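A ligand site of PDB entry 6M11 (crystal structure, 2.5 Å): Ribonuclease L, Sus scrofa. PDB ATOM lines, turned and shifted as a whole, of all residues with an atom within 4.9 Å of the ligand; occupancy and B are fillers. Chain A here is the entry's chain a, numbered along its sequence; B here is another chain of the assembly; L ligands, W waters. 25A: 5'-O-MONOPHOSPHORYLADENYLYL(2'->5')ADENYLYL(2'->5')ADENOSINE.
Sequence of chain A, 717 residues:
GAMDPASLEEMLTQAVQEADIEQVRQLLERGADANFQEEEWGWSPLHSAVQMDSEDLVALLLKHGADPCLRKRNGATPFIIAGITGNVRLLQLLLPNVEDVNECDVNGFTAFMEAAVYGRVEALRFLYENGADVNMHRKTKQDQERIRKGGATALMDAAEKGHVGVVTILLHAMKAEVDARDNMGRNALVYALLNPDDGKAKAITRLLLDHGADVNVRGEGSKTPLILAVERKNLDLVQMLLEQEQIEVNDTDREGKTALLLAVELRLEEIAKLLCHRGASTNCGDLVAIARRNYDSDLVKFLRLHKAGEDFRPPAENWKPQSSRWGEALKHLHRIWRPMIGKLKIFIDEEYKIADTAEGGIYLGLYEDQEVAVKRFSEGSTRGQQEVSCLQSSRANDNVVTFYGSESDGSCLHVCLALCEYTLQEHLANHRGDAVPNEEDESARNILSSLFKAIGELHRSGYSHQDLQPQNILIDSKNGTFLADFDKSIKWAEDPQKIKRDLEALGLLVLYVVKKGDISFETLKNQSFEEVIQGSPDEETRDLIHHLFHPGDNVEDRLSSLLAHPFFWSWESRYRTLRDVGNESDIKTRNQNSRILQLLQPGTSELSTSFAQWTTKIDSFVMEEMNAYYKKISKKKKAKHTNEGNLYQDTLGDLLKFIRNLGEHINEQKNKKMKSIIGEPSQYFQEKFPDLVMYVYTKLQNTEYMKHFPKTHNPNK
Gln 17 touches the ligand (NE2 to N26, 3.8 Å). Trp 41 touches the ligand (CG to OO', 3.4 Å). Ile 84 touches the ligand (CD1 to C12, 3.99 Å). OD2 of Asp 105 touches C2 of the ligand, at 3.7 Å. Phe 109 touches the ligand. Val 117 touches the ligand (CG1 to N6, 3.6 Å). CB of Arg 293 of chain B touches CM' of the ligand (3.8 Å). CE1 of Phe 347 of chain B touches OBP of the ligand, 3.8 Å away. Hydrophobic or aromatic side chains that line the ligand: Trp 41, Trp 43, Ile 84, Phe 109, Val 117, Tyr 118, Tyr 295 of chain B and Phe 347 of chain B.
The backbone carbonyl oxygen of Arg 292 of chain B is in hydrogen-bond range of the side-chain amide nitrogen of Gln 51 (2.8 Å). NZ of Lys 72 sits at hydrogen-bond distance from OH of Tyr 295 of chain B, 3.5 Å away. The side-chain amide oxygen of Asn 74 sits at hydrogen-bond distance from the side-chain amino group of Lys 72. The guanidinium group (NH1) of Arg 292 of chain B is in hydrogen-bond range of the side-chain amide oxygen (OE1) of Gln 17 (3.4 Å). OG of Ser 48 sits close to NE2 of Gln 17 (3.4 Å). N of Trp 43 is in hydrogen-bond range of OE2 of Glu 38. N of Asn 107 is in hydrogen-bond range of OD1 of Asp 105 (2.8 Å). N of Trp 41 sits at hydrogen-bond distance from OE2 of Glu 38 (3.3 Å).
Water W4 lies within hydrogen-bond range of OLP of the ligand (2.7 Å) and O of Arg 293 of chain B (2.9 Å). Water W2 lies within hydrogen-bond range of the side-chain amide nitrogen (ND2) of Asn 107, a nitrogen (N3) of the ligand and the side-chain carboxylate (OD1) of Asp 105. Water W1 lies within hydrogen-bond range of OMP of the ligand (2.9 Å), N of Asn 74 (3.0 Å) and O of Trp 41 (3.0 Å).
A nitrogen (N1) of the ligand sits at hydrogen-bond distance from the side-chain carboxylate of Glu 114, 2.6 Å away. N26 of the ligand lies within hydrogen-bond range of OE1 of Gln 51 (2.6 Å). The side-chain hydroxyl (OH) of Tyr 118 sits at hydrogen-bond distance from a nitrogen (N11) of the ligand (2.7 Å). An oxygen (OLP) of the ligand sits at hydrogen-bond distance from the side-chain hydroxyl (OH) of Tyr 295 of chain B (2.7 Å). The guanidinium group (NH2) of Arg 138 is in salt-bridge range of an oxygen (O1P) of the ligand, at 2.7 Å. An oxygen (OMP) of the ligand is in salt-bridge range of the side-chain amino group of Lys 72 (2.7 Å). NH2 of Arg 338 of chain B lies within salt-bridge range of OCP of the ligand, at 2.8 Å. The guanidinium group (NH1) of Arg 292 of chain B lies within hydrogen-bond range of a nitrogen (N21) of the ligand (2.9 Å). The side-chain hydroxyl of Ser 48 is in hydrogen-bond range of a nitrogen (N26) of the ligand. An oxygen (OMP) of the ligand sits at hydrogen-bond distance from the indole nitrogen (NE1) of Trp 43. An oxygen (O4') of the ligand is in hydrogen-bond range of the side-chain amide nitrogen (ND2) of Asn 107 (3.3 Å). OE' of the ligand lies within hydrogen-bond range of ND2 of Asn 74 (3.5 Å).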
ATOM      1  N   GLN A  17      40.232   5.661 -16.995  1.00  0.00           N
ATOM      2  CA  GLN A  17      39.716   5.170 -18.269  1.00  0.00           C
ATOM      3  C   GLN A  17      40.198   3.767 -18.679  1.00  0.00           C
ATOM      4  O   GLN A  17      39.422   3.004 -19.254  1.00  0.00           O
ATOM      5  CB  GLN A  17      39.968   6.213 -19.379  1.00  0.00           C
ATOM      6  CG  GLN A  17      39.125   7.491 -19.232  1.00  0.00           C
ATOM      7  CD  GLN A  17      37.613   7.251 -19.364  1.00  0.00           C
ATOM      8  OE1 GLN A  17      37.156   6.696 -20.363  1.00  0.00           O
ATOM      9  NE2 GLN A  17      36.866   7.621 -18.329  1.00  0.00           N
ATOM     10  N   GLU A  38      38.071  18.203 -16.217  1.00  0.00           N
ATOM     11  CA  GLU A  38      38.426  18.697 -17.560  1.00  0.00           C
ATOM     12  C   GLU A  38      37.508  19.843 -17.967  1.00  0.00           C
ATOM     13  O   GLU A  38      36.303  19.811 -17.712  1.00  0.00           O
ATOM     14  CB  GLU A  38      38.529  17.596 -18.632  1.00  0.00           C
ATOM     15  CG  GLU A  38      37.361  16.632 -18.710  1.00  0.00           C
ATOM     16  CD  GLU A  38      36.229  17.059 -19.649  1.00  0.00           C
ATOM     17  OE1 GLU A  38      36.495  17.597 -20.756  1.00  0.00           O
ATOM     18  OE2 GLU A  38      35.084  16.745 -19.309  1.00  0.00           O
ATOM     19  N   TRP A  41      33.740  19.447 -20.646  1.00  0.00           N
ATOM     20  CA  TRP A  41      32.431  18.901 -20.264  1.00  0.00           C
ATOM     21  C   TRP A  41      32.278  18.681 -18.774  1.00  0.00           C
ATOM     22  O   TRP A  41      31.269  18.112 -18.327  1.00  0.00           O
ATOM     23  CB  TRP A  41      32.187  17.625 -21.022  1.00  0.00           C
ATOM     24  CG  TRP A  41      32.079  17.795 -22.487  1.00  0.00           C
ATOM     25  CD1 TRP A  41      32.992  17.438 -23.394  1.00  0.00           C
ATOM     26  CD2 TRP A  41      31.000  18.410 -23.198  1.00  0.00           C
ATOM     27  NE1 TRP A  41      32.561  17.751 -24.672  1.00  0.00           N
ATOM     28  CE2 TRP A  41      31.333  18.344 -24.574  1.00  0.00           C
ATOM     29  CE3 TRP A  41      29.784  18.994 -22.824  1.00  0.00           C
ATOM     30  CZ2 TRP A  41      30.482  18.841 -25.589  1.00  0.00           C
ATOM     31  CZ3 TRP A  41      28.941  19.504 -23.811  1.00  0.00           C
ATOM     32  CH2 TRP A  41      29.298  19.419 -25.185  1.00  0.00           C
ATOM     33  N   TRP A  43      33.788  16.601 -16.576  1.00  0.00           N
ATOM     34  CA  TRP A  43      33.918  15.241 -16.047  1.00  0.00           C
ATOM     35  C   TRP A  43      35.097  15.109 -15.069  1.00  0.00           C
ATOM     36  O   TRP A  43      36.194  15.614 -15.338  1.00  0.00           O
ATOM     37  CB  TRP A  43      34.071  14.230 -17.205  1.00  0.00           C
ATOM     38  CG  TRP A  43      32.770  13.980 -17.927  1.00  0.00           C
ATOM     39  CD1 TRP A  43      32.172  14.792 -18.867  1.00  0.00           C
ATOM     40  CD2 TRP A  43      31.883  12.872 -17.737  1.00  0.00           C
ATOM     41  NE1 TRP A  43      30.988  14.253 -19.277  1.00  0.00           N
ATOM     42  CE2 TRP A  43      30.784  13.068 -18.612  1.00  0.00           C
ATOM     43  CE3 TRP A  43      31.917  11.729 -16.943  1.00  0.00           C
ATOM     44  CZ2 TRP A  43      29.720  12.165 -18.692  1.00  0.00           C
ATOM     45  CZ3 TRP A  43      30.853  10.826 -17.024  1.00  0.00           C
ATOM     46  CH2 TRP A  43      29.768  11.052 -17.902  1.00  0.00           C
ATOM     47  N   SER A  48      33.672   9.566 -14.007  1.00  0.00           N
ATOM     48  CA  SER A  48      34.121   8.545 -14.961  1.00  0.00           C
ATOM     49  C   SER A  48      34.125   7.120 -14.441  1.00  0.00           C
ATOM     50  O   SER A  48      33.778   6.181 -15.171  1.00  0.00           O
ATOM     51  CB  SER A  48      35.499   8.906 -15.509  1.00  0.00           C
ATOM     52  OG  SER A  48      35.387   9.996 -16.387  1.00  0.00           O
ATOM     53  N   GLN A  51      30.395   5.949 -14.288  1.00  0.00           N
ATOM     54  CA  GLN A  51      29.924   5.641 -15.645  1.00  0.00           C
ATOM     55  C   GLN A  51      30.408   4.295 -16.245  1.00  0.00           C
ATOM     56  O   GLN A  51      29.660   3.611 -16.949  1.00  0.00           O
ATOM     57  CB  GLN A  51      30.250   6.796 -16.591  1.00  0.00           C
ATOM     58  CG  GLN A  51      29.919   6.588 -18.061  1.00  0.00           C
ATOM     59  CD  GLN A  51      30.572   7.631 -18.934  1.00  0.00           C
ATOM     60  OE1 GLN A  51      31.782   7.822 -18.870  1.00  0.00           O
ATOM     61  NE2 GLN A  51      29.780   8.307 -19.770  1.00  0.00           N
ATOM     62  N   LYS A  72      29.288  18.212 -13.104  1.00  0.00           N
ATOM     63  CA  LYS A  72      29.845  18.409 -14.470  1.00  0.00           C
ATOM     64  C   LYS A  72      29.114  19.506 -15.258  1.00  0.00           C
ATOM     65  O   LYS A  72      28.334  20.262 -14.675  1.00  0.00           O
ATOM     66  CB  LYS A  72      29.987  17.085 -15.228  1.00  0.00           C
ATOM     67  CG  LYS A  72      28.789  16.161 -15.347  1.00  0.00           C
ATOM     68  CD  LYS A  72      29.235  14.874 -16.034  1.00  0.00           C
ATOM     69  CE  LYS A  72      28.105  13.921 -16.369  1.00  0.00           C
ATOM     70  NZ  LYS A  72      27.076  14.420 -17.358  1.00  0.00           N
ATOM     71  N   ASN A  74      26.591  19.702 -17.399  1.00  0.00           N
ATOM     72  CA  ASN A  74      25.140  19.591 -17.270  1.00  0.00           C
ATOM     73  C   ASN A  74      24.596  19.599 -15.823  1.00  0.00           C
ATOM     74  O   ASN A  74      23.393  19.393 -15.607  1.00  0.00           O
ATOM     75  CB  ASN A  74      24.620  18.354 -18.064  1.00  0.00           C
ATOM     76  CG  ASN A  74      24.994  17.004 -17.426  1.00  0.00           C
ATOM     77  OD1 ASN A  74      25.947  16.891 -16.644  1.00  0.00           O
ATOM     78  ND2 ASN A  74      24.236  15.952 -17.786  1.00  0.00           N
ATOM     79  N   ILE A  84      21.852   6.035 -13.867  1.00  0.00           N
ATOM     80  CA  ILE A  84      22.054   5.613 -15.257  1.00  0.00           C
ATOM     81  C   ILE A  84      22.833   4.286 -15.252  1.00  0.00           C
ATOM     82  O   ILE A  84      22.463   3.353 -15.936  1.00  0.00           O
ATOM     83  CB  ILE A  84      22.843   6.708 -16.043  1.00  0.00           C
ATOM     84  CG1 ILE A  84      22.114   8.053 -15.985  1.00  0.00           C
ATOM     85  CG2 ILE A  84      23.143   6.281 -17.473  1.00  0.00           C
ATOM     86  CD1 ILE A  84      22.944   9.290 -16.223  1.00  0.00           C
ATOM     87  N   ASP A 105      20.320  17.724 -12.003  1.00  0.00           N
ATOM     88  CA  ASP A 105      21.147  18.438 -12.982  1.00  0.00           C
ATOM     89  C   ASP A 105      20.441  19.673 -13.562  1.00  0.00           C
ATOM     90  O   ASP A 105      19.330  19.952 -13.169  1.00  0.00           O
ATOM     91  CB  ASP A 105      21.762  17.461 -14.014  1.00  0.00           C
ATOM     92  CG  ASP A 105      20.807  16.999 -15.104  1.00  0.00           C
ATOM     93  OD1 ASP A 105      19.927  17.764 -15.553  1.00  0.00           O
ATOM     94  OD2 ASP A 105      20.931  15.801 -15.511  1.00  0.00           O
ATOM     95  N   ASN A 107      18.896  20.305 -16.250  1.00  0.00           N
ATOM     96  CA  ASN A 107      17.657  19.974 -16.975  1.00  0.00           C
ATOM     97  C   ASN A 107      16.591  19.297 -16.097  1.00  0.00           C
ATOM     98  O   ASN A 107      15.652  18.694 -16.589  1.00  0.00           O
ATOM     99  CB  ASN A 107      17.973  19.150 -18.221  1.00  0.00           C
ATOM    100  CG  ASN A 107      18.771  19.927 -19.269  1.00  0.00           C
ATOM    101  OD1 ASN A 107      18.305  20.926 -19.804  1.00  0.00           O
ATOM    102  ND2 ASN A 107      19.986  19.475 -19.559  1.00  0.00           N
ATOM    103  N   PHE A 109      16.865  16.601 -14.122  1.00  0.00           N
ATOM    104  CA  PHE A 109      17.039  15.159 -13.958  1.00  0.00           C
ATOM    105  C   PHE A 109      17.597  14.752 -12.562  1.00  0.00           C
ATOM    106  O   PHE A 109      18.533  15.382 -12.075  1.00  0.00           O
ATOM    107  CB  PHE A 109      17.918  14.622 -15.058  1.00  0.00           C
ATOM    108  CG  PHE A 109      17.201  14.310 -16.349  1.00  0.00           C
ATOM    109  CD1 PHE A 109      17.068  15.281 -17.338  1.00  0.00           C
ATOM    110  CD2 PHE A 109      16.740  13.019 -16.602  1.00  0.00           C
ATOM    111  CE1 PHE A 109      16.420  15.000 -18.546  1.00  0.00           C
ATOM    112  CE2 PHE A 109      16.100  12.717 -17.810  1.00  0.00           C
ATOM    113  CZ  PHE A 109      15.951  13.711 -18.783  1.00  0.00           C
ATOM    114  N   GLU A 114      16.790   9.159 -13.850  1.00  0.00           N
ATOM    115  CA  GLU A 114      17.823   8.445 -14.604  1.00  0.00           C
ATOM    116  C   GLU A 114      17.721   6.963 -14.502  1.00  0.00           C
ATOM    117  O   GLU A 114      17.928   6.311 -15.523  1.00  0.00           O
ATOM    118  CB  GLU A 114      19.213   8.896 -14.226  1.00  0.00           C
ATOM    119  CG  GLU A 114      19.465  10.380 -14.468  1.00  0.00           C
ATOM    120  CD  GLU A 114      19.585  10.751 -15.944  1.00  0.00           C
ATOM    121  OE1 GLU A 114      19.311   9.902 -16.840  1.00  0.00           O
ATOM    122  OE2 GLU A 114      19.938  11.933 -16.188  1.00  0.00           O
ATOM    123  N   VAL A 117      14.689   6.245 -16.871  1.00  0.00           N
ATOM    124  CA  VAL A 117      15.145   6.377 -18.259  1.00  0.00           C
ATOM    125  C   VAL A 117      15.928   5.118 -18.681  1.00  0.00           C
ATOM    126  O   VAL A 117      15.768   4.616 -19.785  1.00  0.00           O
ATOM    127  CB  VAL A 117      15.980   7.697 -18.520  1.00  0.00           C
ATOM    128  CG1 VAL A 117      16.543   7.723 -19.916  1.00  0.00           C
ATOM    129  CG2 VAL A 117      15.117   8.940 -18.469  1.00  0.00           C
ATOM    130  N   TYR A 118      16.759   4.570 -17.806  1.00  0.00           N
ATOM    131  CA  TYR A 118      17.579   3.459 -18.263  1.00  0.00           C
ATOM    132  C   TYR A 118      17.042   2.062 -17.957  1.00  0.00           C
ATOM    133  O   TYR A 118      17.687   1.070 -18.280  1.00  0.00           O
ATOM    134  CB  TYR A 118      19.046   3.634 -17.857  1.00  0.00           C
ATOM    135  CG  TYR A 118      19.739   4.724 -18.659  1.00  0.00           C
ATOM    136  CD1 TYR A 118      19.634   6.074 -18.266  1.00  0.00           C
ATOM    137  CD2 TYR A 118      20.450   4.427 -19.821  1.00  0.00           C
ATOM    138  CE1 TYR A 118      20.232   7.071 -19.017  1.00  0.00           C
ATOM    139  CE2 TYR A 118      21.032   5.422 -20.574  1.00  0.00           C
ATOM    140  CZ  TYR A 118      20.942   6.725 -20.166  1.00  0.00           C
ATOM    141  OH  TYR A 118      21.553   7.717 -20.910  1.00  0.00           O
ATOM    142  N   ARG A 138      10.536  17.593 -13.813  1.00  0.00           N
ATOM    143  CA  ARG A 138      11.837  18.276 -14.050  1.00  0.00           C
ATOM    144  C   ARG A 138      11.714  19.796 -14.063  1.00  0.00           C
ATOM    145  O   ARG A 138      10.916  20.343 -14.817  1.00  0.00           O
ATOM    146  CB  ARG A 138      12.500  17.806 -15.329  1.00  0.00           C
ATOM    147  CG  ARG A 138      12.642  16.341 -15.445  1.00  0.00           C
ATOM    148  CD  ARG A 138      13.744  16.053 -16.391  1.00  0.00           C
ATOM    149  NE  ARG A 138      13.247  15.678 -17.705  1.00  0.00           N
ATOM    150  CZ  ARG A 138      12.784  14.480 -18.037  1.00  0.00           C
ATOM    151  NH1 ARG A 138      12.645  13.528 -17.105  1.00  0.00           N
ATOM    152  NH2 ARG A 138      12.409  14.234 -19.276  1.00  0.00           N
ATOM    153  N   LYS A 149       9.159  23.876 -22.176  1.00  0.00           N
ATOM    154  CA  LYS A 149       9.851  22.567 -22.036  1.00  0.00           C
ATOM    155  C   LYS A 149       9.974  22.162 -20.555  1.00  0.00           C
ATOM    156  O   LYS A 149       9.783  22.999 -19.672  1.00  0.00           O
ATOM    157  CB  LYS A 149      11.218  22.566 -22.720  1.00  0.00           C
ATOM    158  CG  LYS A 149      11.255  21.869 -24.067  1.00  0.00           C
ATOM    159  CD  LYS A 149      12.718  21.596 -24.420  1.00  0.00           C
ATOM    160  CE  LYS A 149      12.910  20.378 -25.325  1.00  0.00           C
ATOM    161  NZ  LYS A 149      12.480  20.682 -26.719  1.00  0.00           N
ATOM    162  N   GLY A 150      10.317  20.896 -20.318  1.00  0.00           N
ATOM    163  CA  GLY A 150      10.430  20.310 -18.985  1.00  0.00           C
ATOM    164  C   GLY A 150       9.119  19.789 -18.398  1.00  0.00           C
ATOM    165  O   GLY A 150       8.138  19.595 -19.110  1.00  0.00           O
ATOM    166  N   ARG B 292      30.951   5.213 -24.825  1.00  0.00           N
ATOM    167  CA  ARG B 292      31.090   5.935 -23.555  1.00  0.00           C
ATOM    168  C   ARG B 292      30.050   7.064 -23.368  1.00  0.00           C
ATOM    169  O   ARG B 292      29.496   7.195 -22.284  1.00  0.00           O
ATOM    170  CB  ARG B 292      32.530   6.451 -23.383  1.00  0.00           C
ATOM    171  CG  ARG B 292      32.843   7.129 -22.057  1.00  0.00           C
ATOM    172  CD  ARG B 292      34.274   7.608 -22.034  1.00  0.00           C
ATOM    173  NE  ARG B 292      34.399   8.895 -22.729  1.00  0.00           N
ATOM    174  CZ  ARG B 292      35.250   9.852 -22.419  1.00  0.00           C
ATOM    175  NH1 ARG B 292      36.105   9.704 -21.400  1.00  0.00           N
ATOM    176  NH2 ARG B 292      35.246  10.996 -23.112  1.00  0.00           N
ATOM    177  N   ARG B 293      29.802   7.877 -24.405  1.00  0.00           N
ATOM    178  CA  ARG B 293      28.805   8.953 -24.286  1.00  0.00           C
ATOM    179  C   ARG B 293      27.381   8.428 -24.325  1.00  0.00           C
ATOM    180  O   ARG B 293      26.453   9.069 -23.807  1.00  0.00           O
ATOM    181  CB  ARG B 293      29.004  10.079 -25.319  1.00  0.00           C
ATOM    182  CG  ARG B 293      28.707   9.708 -26.754  1.00  0.00           C
ATOM    183  CD  ARG B 293      28.160  10.832 -27.603  1.00  0.00           C
ATOM    184  NE  ARG B 293      27.994  10.342 -28.974  1.00  0.00           N
ATOM    185  CZ  ARG B 293      28.937  10.399 -29.920  1.00  0.00           C
ATOM    186  NH1 ARG B 293      30.132  10.919 -29.651  1.00  0.00           N
ATOM    187  NH2 ARG B 293      28.690   9.897 -31.128  1.00  0.00           N
ATOM    188  N   TYR B 295      26.454   6.039 -22.614  1.00  0.00           N
ATOM    189  CA  TYR B 295      26.486   5.278 -21.355  1.00  0.00           C
ATOM    190  C   TYR B 295      26.364   3.748 -21.557  1.00  0.00           C
ATOM    191  O   TYR B 295      25.662   3.086 -20.822  1.00  0.00           O
ATOM    192  CB  TYR B 295      25.525   5.824 -20.272  1.00  0.00           C
ATOM    193  CG  TYR B 295      25.734   7.286 -19.833  1.00  0.00           C
ATOM    194  CD1 TYR B 295      25.266   8.343 -20.625  1.00  0.00           C
ATOM    195  CD2 TYR B 295      26.376   7.619 -18.622  1.00  0.00           C
ATOM    196  CE1 TYR B 295      25.433   9.685 -20.262  1.00  0.00           C
ATOM    197  CE2 TYR B 295      26.555   8.956 -18.252  1.00  0.00           C
ATOM    198  CZ  TYR B 295      26.106   9.985 -19.083  1.00  0.00           C
ATOM    199  OH  TYR B 295      26.251  11.318 -18.716  1.00  0.00           O
ATOM    200  N   TRP B 337      30.193  17.034 -30.361  1.00  0.00           N
ATOM    201  CA  TRP B 337      29.201  16.132 -30.947  1.00  0.00           C
ATOM    202  C   TRP B 337      27.833  16.563 -30.465  1.00  0.00           C
ATOM    203  O   TRP B 337      27.630  16.837 -29.270  1.00  0.00           O
ATOM    204  CB  TRP B 337      29.433  14.646 -30.629  1.00  0.00           C
ATOM    205  CG  TRP B 337      28.388  13.770 -31.240  1.00  0.00           C
ATOM    206  CD1 TRP B 337      28.400  13.214 -32.517  1.00  0.00           C
ATOM    207  CD2 TRP B 337      27.163  13.342 -30.630  1.00  0.00           C
ATOM    208  NE1 TRP B 337      27.249  12.460 -32.716  1.00  0.00           N
ATOM    209  CE2 TRP B 337      26.471  12.513 -31.584  1.00  0.00           C
ATOM    210  CE3 TRP B 337      26.559  13.576 -29.370  1.00  0.00           C
ATOM    211  CZ2 TRP B 337      25.196  11.933 -31.316  1.00  0.00           C
ATOM    212  CZ3 TRP B 337      25.275  12.968 -29.091  1.00  0.00           C
ATOM    213  CH2 TRP B 337      24.624  12.159 -30.072  1.00  0.00           C
ATOM    214  N   ARG B 338      26.901  16.659 -31.416  1.00  0.00           N
ATOM    215  CA  ARG B 338      25.521  16.910 -31.103  1.00  0.00           C
ATOM    216  C   ARG B 338      24.667  15.995 -31.970  1.00  0.00           C
ATOM    217  O   ARG B 338      25.075  15.579 -33.066  1.00  0.00           O
ATOM    218  CB  ARG B 338      25.136  18.377 -31.333  1.00  0.00           C
ATOM    219  CG  ARG B 338      25.761  19.434 -30.400  1.00  0.00           C
ATOM    220  CD  ARG B 338      25.399  19.270 -28.927  1.00  0.00           C
ATOM    221  NE  ARG B 338      23.966  19.143 -28.781  1.00  0.00           N
ATOM    222  CZ  ARG B 338      23.296  18.565 -27.782  1.00  0.00           C
ATOM    223  NH1 ARG B 338      23.921  18.066 -26.737  1.00  0.00           N
ATOM    224  NH2 ARG B 338      21.970  18.461 -27.898  1.00  0.00           N
ATOM    225  N   PHE B 347      23.209  23.502 -29.503  1.00  0.00           N
ATOM    226  CA  PHE B 347      23.437  23.189 -28.126  1.00  0.00           C
ATOM    227  C   PHE B 347      22.949  24.326 -27.261  1.00  0.00           C
ATOM    228  O   PHE B 347      23.355  25.443 -27.495  1.00  0.00           O
ATOM    229  CB  PHE B 347      24.924  22.893 -27.914  1.00  0.00           C
ATOM    230  CG  PHE B 347      25.242  22.409 -26.532  1.00  0.00           C
ATOM    231  CD1 PHE B 347      24.308  21.609 -25.823  1.00  0.00           C
ATOM    232  CD2 PHE B 347      26.454  22.716 -25.915  1.00  0.00           C
ATOM    233  CE1 PHE B 347      24.588  21.145 -24.541  1.00  0.00           C
ATOM    234  CE2 PHE B 347      26.730  22.236 -24.639  1.00  0.00           C
ATOM    235  CZ  PHE B 347      25.806  21.464 -23.943  1.00  0.00           C
HETATM  236  O1P 25A L   1      13.294  15.152 -21.666  1.00  0.00           O
HETATM  237  P   25A L   1      13.576  16.629 -21.480  1.00  0.00           P
HETATM  238  O2P 25A L   1      12.743  17.418 -22.601  1.00  0.00           O
HETATM  239  O3P 25A L   1      13.336  17.412 -20.183  1.00  0.00           O
HETATM  240  O5' 25A L   1      15.153  16.751 -21.866  1.00  0.00           O
HETATM  241  C5' 25A L   1      15.903  17.904 -21.433  1.00  0.00           C
HETATM  242  C4' 25A L   1      17.310  17.913 -22.013  1.00  0.00           C
HETATM  243  O4' 25A L   1      18.248  17.174 -21.205  1.00  0.00           O
HETATM  244  C1' 25A L   1      19.080  16.377 -22.063  1.00  0.00           C
HETATM  245  C2' 25A L   1      18.796  16.767 -23.499  1.00  0.00           C
HETATM  246  O2' 25A L   1      19.620  17.889 -23.657  1.00  0.00           O
HETATM  247  C3' 25A L   1      17.377  17.303 -23.411  1.00  0.00           C
HETATM  248  O3' 25A L   1      17.076  18.365 -24.296  1.00  0.00           O
HETATM  249  N9  25A L   1      18.737  14.974 -21.768  1.00  0.00           N
HETATM  250  C8  25A L   1      17.985  14.148 -22.492  1.00  0.00           C
HETATM  251  N7  25A L   1      17.921  12.939 -21.908  1.00  0.00           N
HETATM  252  C5  25A L   1      18.614  13.015 -20.777  1.00  0.00           C
HETATM  253  C6  25A L   1      18.913  12.079 -19.689  1.00  0.00           C
HETATM  254  N6  25A L   1      18.420  10.831 -19.749  1.00  0.00           N
HETATM  255  C4  25A L   1      19.180  14.356 -20.687  1.00  0.00           C
HETATM  256  N3  25A L   1      19.961  14.743 -19.636  1.00  0.00           N
HETATM  257  C2  25A L   1      20.291  13.839 -18.550  1.00  0.00           C
HETATM  258  N1  25A L   1      19.698  12.485 -18.691  1.00  0.00           N
HETATM  259  P1  25A L   1      20.991  18.056 -24.409  1.00  0.00           P
HETATM  260  OBP 25A L   1      21.111  19.560 -24.375  1.00  0.00           O
HETATM  261  OCP 25A L   1      20.965  17.165 -25.604  1.00  0.00           O
HETATM  262  OF' 25A L   1      22.046  17.453 -23.373  1.00  0.00           O
HETATM  263  CF' 25A L   1      22.736  18.276 -22.452  1.00  0.00           C
HETATM  264  CE' 25A L   1      23.752  17.356 -21.793  1.00  0.00           C
HETATM  265  OE' 25A L   1      23.101  16.309 -21.048  1.00  0.00           O
HETATM  266  CB' 25A L   1      23.789  15.069 -21.214  1.00  0.00           C
HETATM  267  N19 25A L   1      22.857  14.093 -21.837  1.00  0.00           N
HETATM  268  C18 25A L   1      22.189  14.224 -22.999  1.00  0.00           C
HETATM  269  N17 25A L   1      21.438  13.126 -23.271  1.00  0.00           N
HETATM  270  C15 25A L   1      21.598  12.307 -22.219  1.00  0.00           C
HETATM  271  C14 25A L   1      22.525  12.941 -21.274  1.00  0.00           C
HETATM  272  N13 25A L   1      22.903  12.328 -20.136  1.00  0.00           N
HETATM  273  C12 25A L   1      22.425  11.018 -19.780  1.00  0.00           C
HETATM  274  N11 25A L   1      21.484  10.398 -20.721  1.00  0.00           N
HETATM  275  C16 25A L   1      21.080  10.982 -21.849  1.00  0.00           C
HETATM  276  N16 25A L   1      20.234  10.332 -22.659  1.00  0.00           N
HETATM  277  CC' 25A L   1      24.999  15.328 -22.088  1.00  0.00           C
HETATM  278  OC' 25A L   1      26.070  15.464 -21.165  1.00  0.00           O
HETATM  279  CD' 25A L   1      24.742  16.681 -22.732  1.00  0.00           C
HETATM  280  OD' 25A L   1      25.896  17.514 -22.648  1.00  0.00           O
HETATM  281  P2  25A L   1      27.247  14.387 -20.904  1.00  0.00           P
HETATM  282  OLP 25A L   1      26.546  13.048 -20.769  1.00  0.00           O
HETATM  283  OMP 25A L   1      27.990  15.116 -19.824  1.00  0.00           O
HETATM  284  OP' 25A L   1      28.048  14.367 -22.278  1.00  0.00           O
HETATM  285  CP' 25A L   1      28.677  15.545 -22.753  1.00  0.00           C
HETATM  286  CO' 25A L   1      29.900  15.067 -23.472  1.00  0.00           C
HETATM  287  OO' 25A L   1      30.892  14.633 -22.538  1.00  0.00           O
HETATM  288  CL' 25A L   1      31.684  13.635 -23.183  1.00  0.00           C
HETATM  289  N29 25A L   1      31.921  12.541 -22.208  1.00  0.00           N
HETATM  290  C28 25A L   1      31.090  11.506 -21.974  1.00  0.00           C
HETATM  291  N27 25A L   1      31.596  10.690 -21.042  1.00  0.00           N
HETATM  292  C25 25A L   1      32.780  11.190 -20.645  1.00  0.00           C
HETATM  293  C24 25A L   1      32.989  12.421 -21.406  1.00  0.00           C
HETATM  294  N23 25A L   1      34.130  13.128 -21.225  1.00  0.00           N
HETATM  295  C22 25A L   1      35.199  12.783 -20.285  1.00  0.00           C
HETATM  296  N21 25A L   1      34.955  11.547 -19.527  1.00  0.00           N
HETATM  297  C26 25A L   1      33.828  10.785 -19.667  1.00  0.00           C
HETATM  298  N26 25A L   1      33.675   9.647 -18.936  1.00  0.00           N
HETATM  299  CM' 25A L   1      30.945  13.171 -24.424  1.00  0.00           C
HETATM  300  OM' 25A L   1      31.668  13.606 -25.591  1.00  0.00           O
HETATM  301  CN' 25A L   1      29.600  13.849 -24.319  1.00  0.00           C
HETATM  302  ON' 25A L   1      29.047  14.259 -25.556  1.00  0.00           O
HETATM  303  O   HOH W   1      28.361  17.863 -18.899  1.00  0.00           O
HETATM  304  O   HOH W   2      20.977  17.154 -18.464  1.00  0.00           O
HETATM  305  O   HOH W   3      21.603  21.990 -23.028  1.00  0.00           O
HETATM  306  O   HOH W   4      27.509  11.540 -22.754  1.00  0.00           O
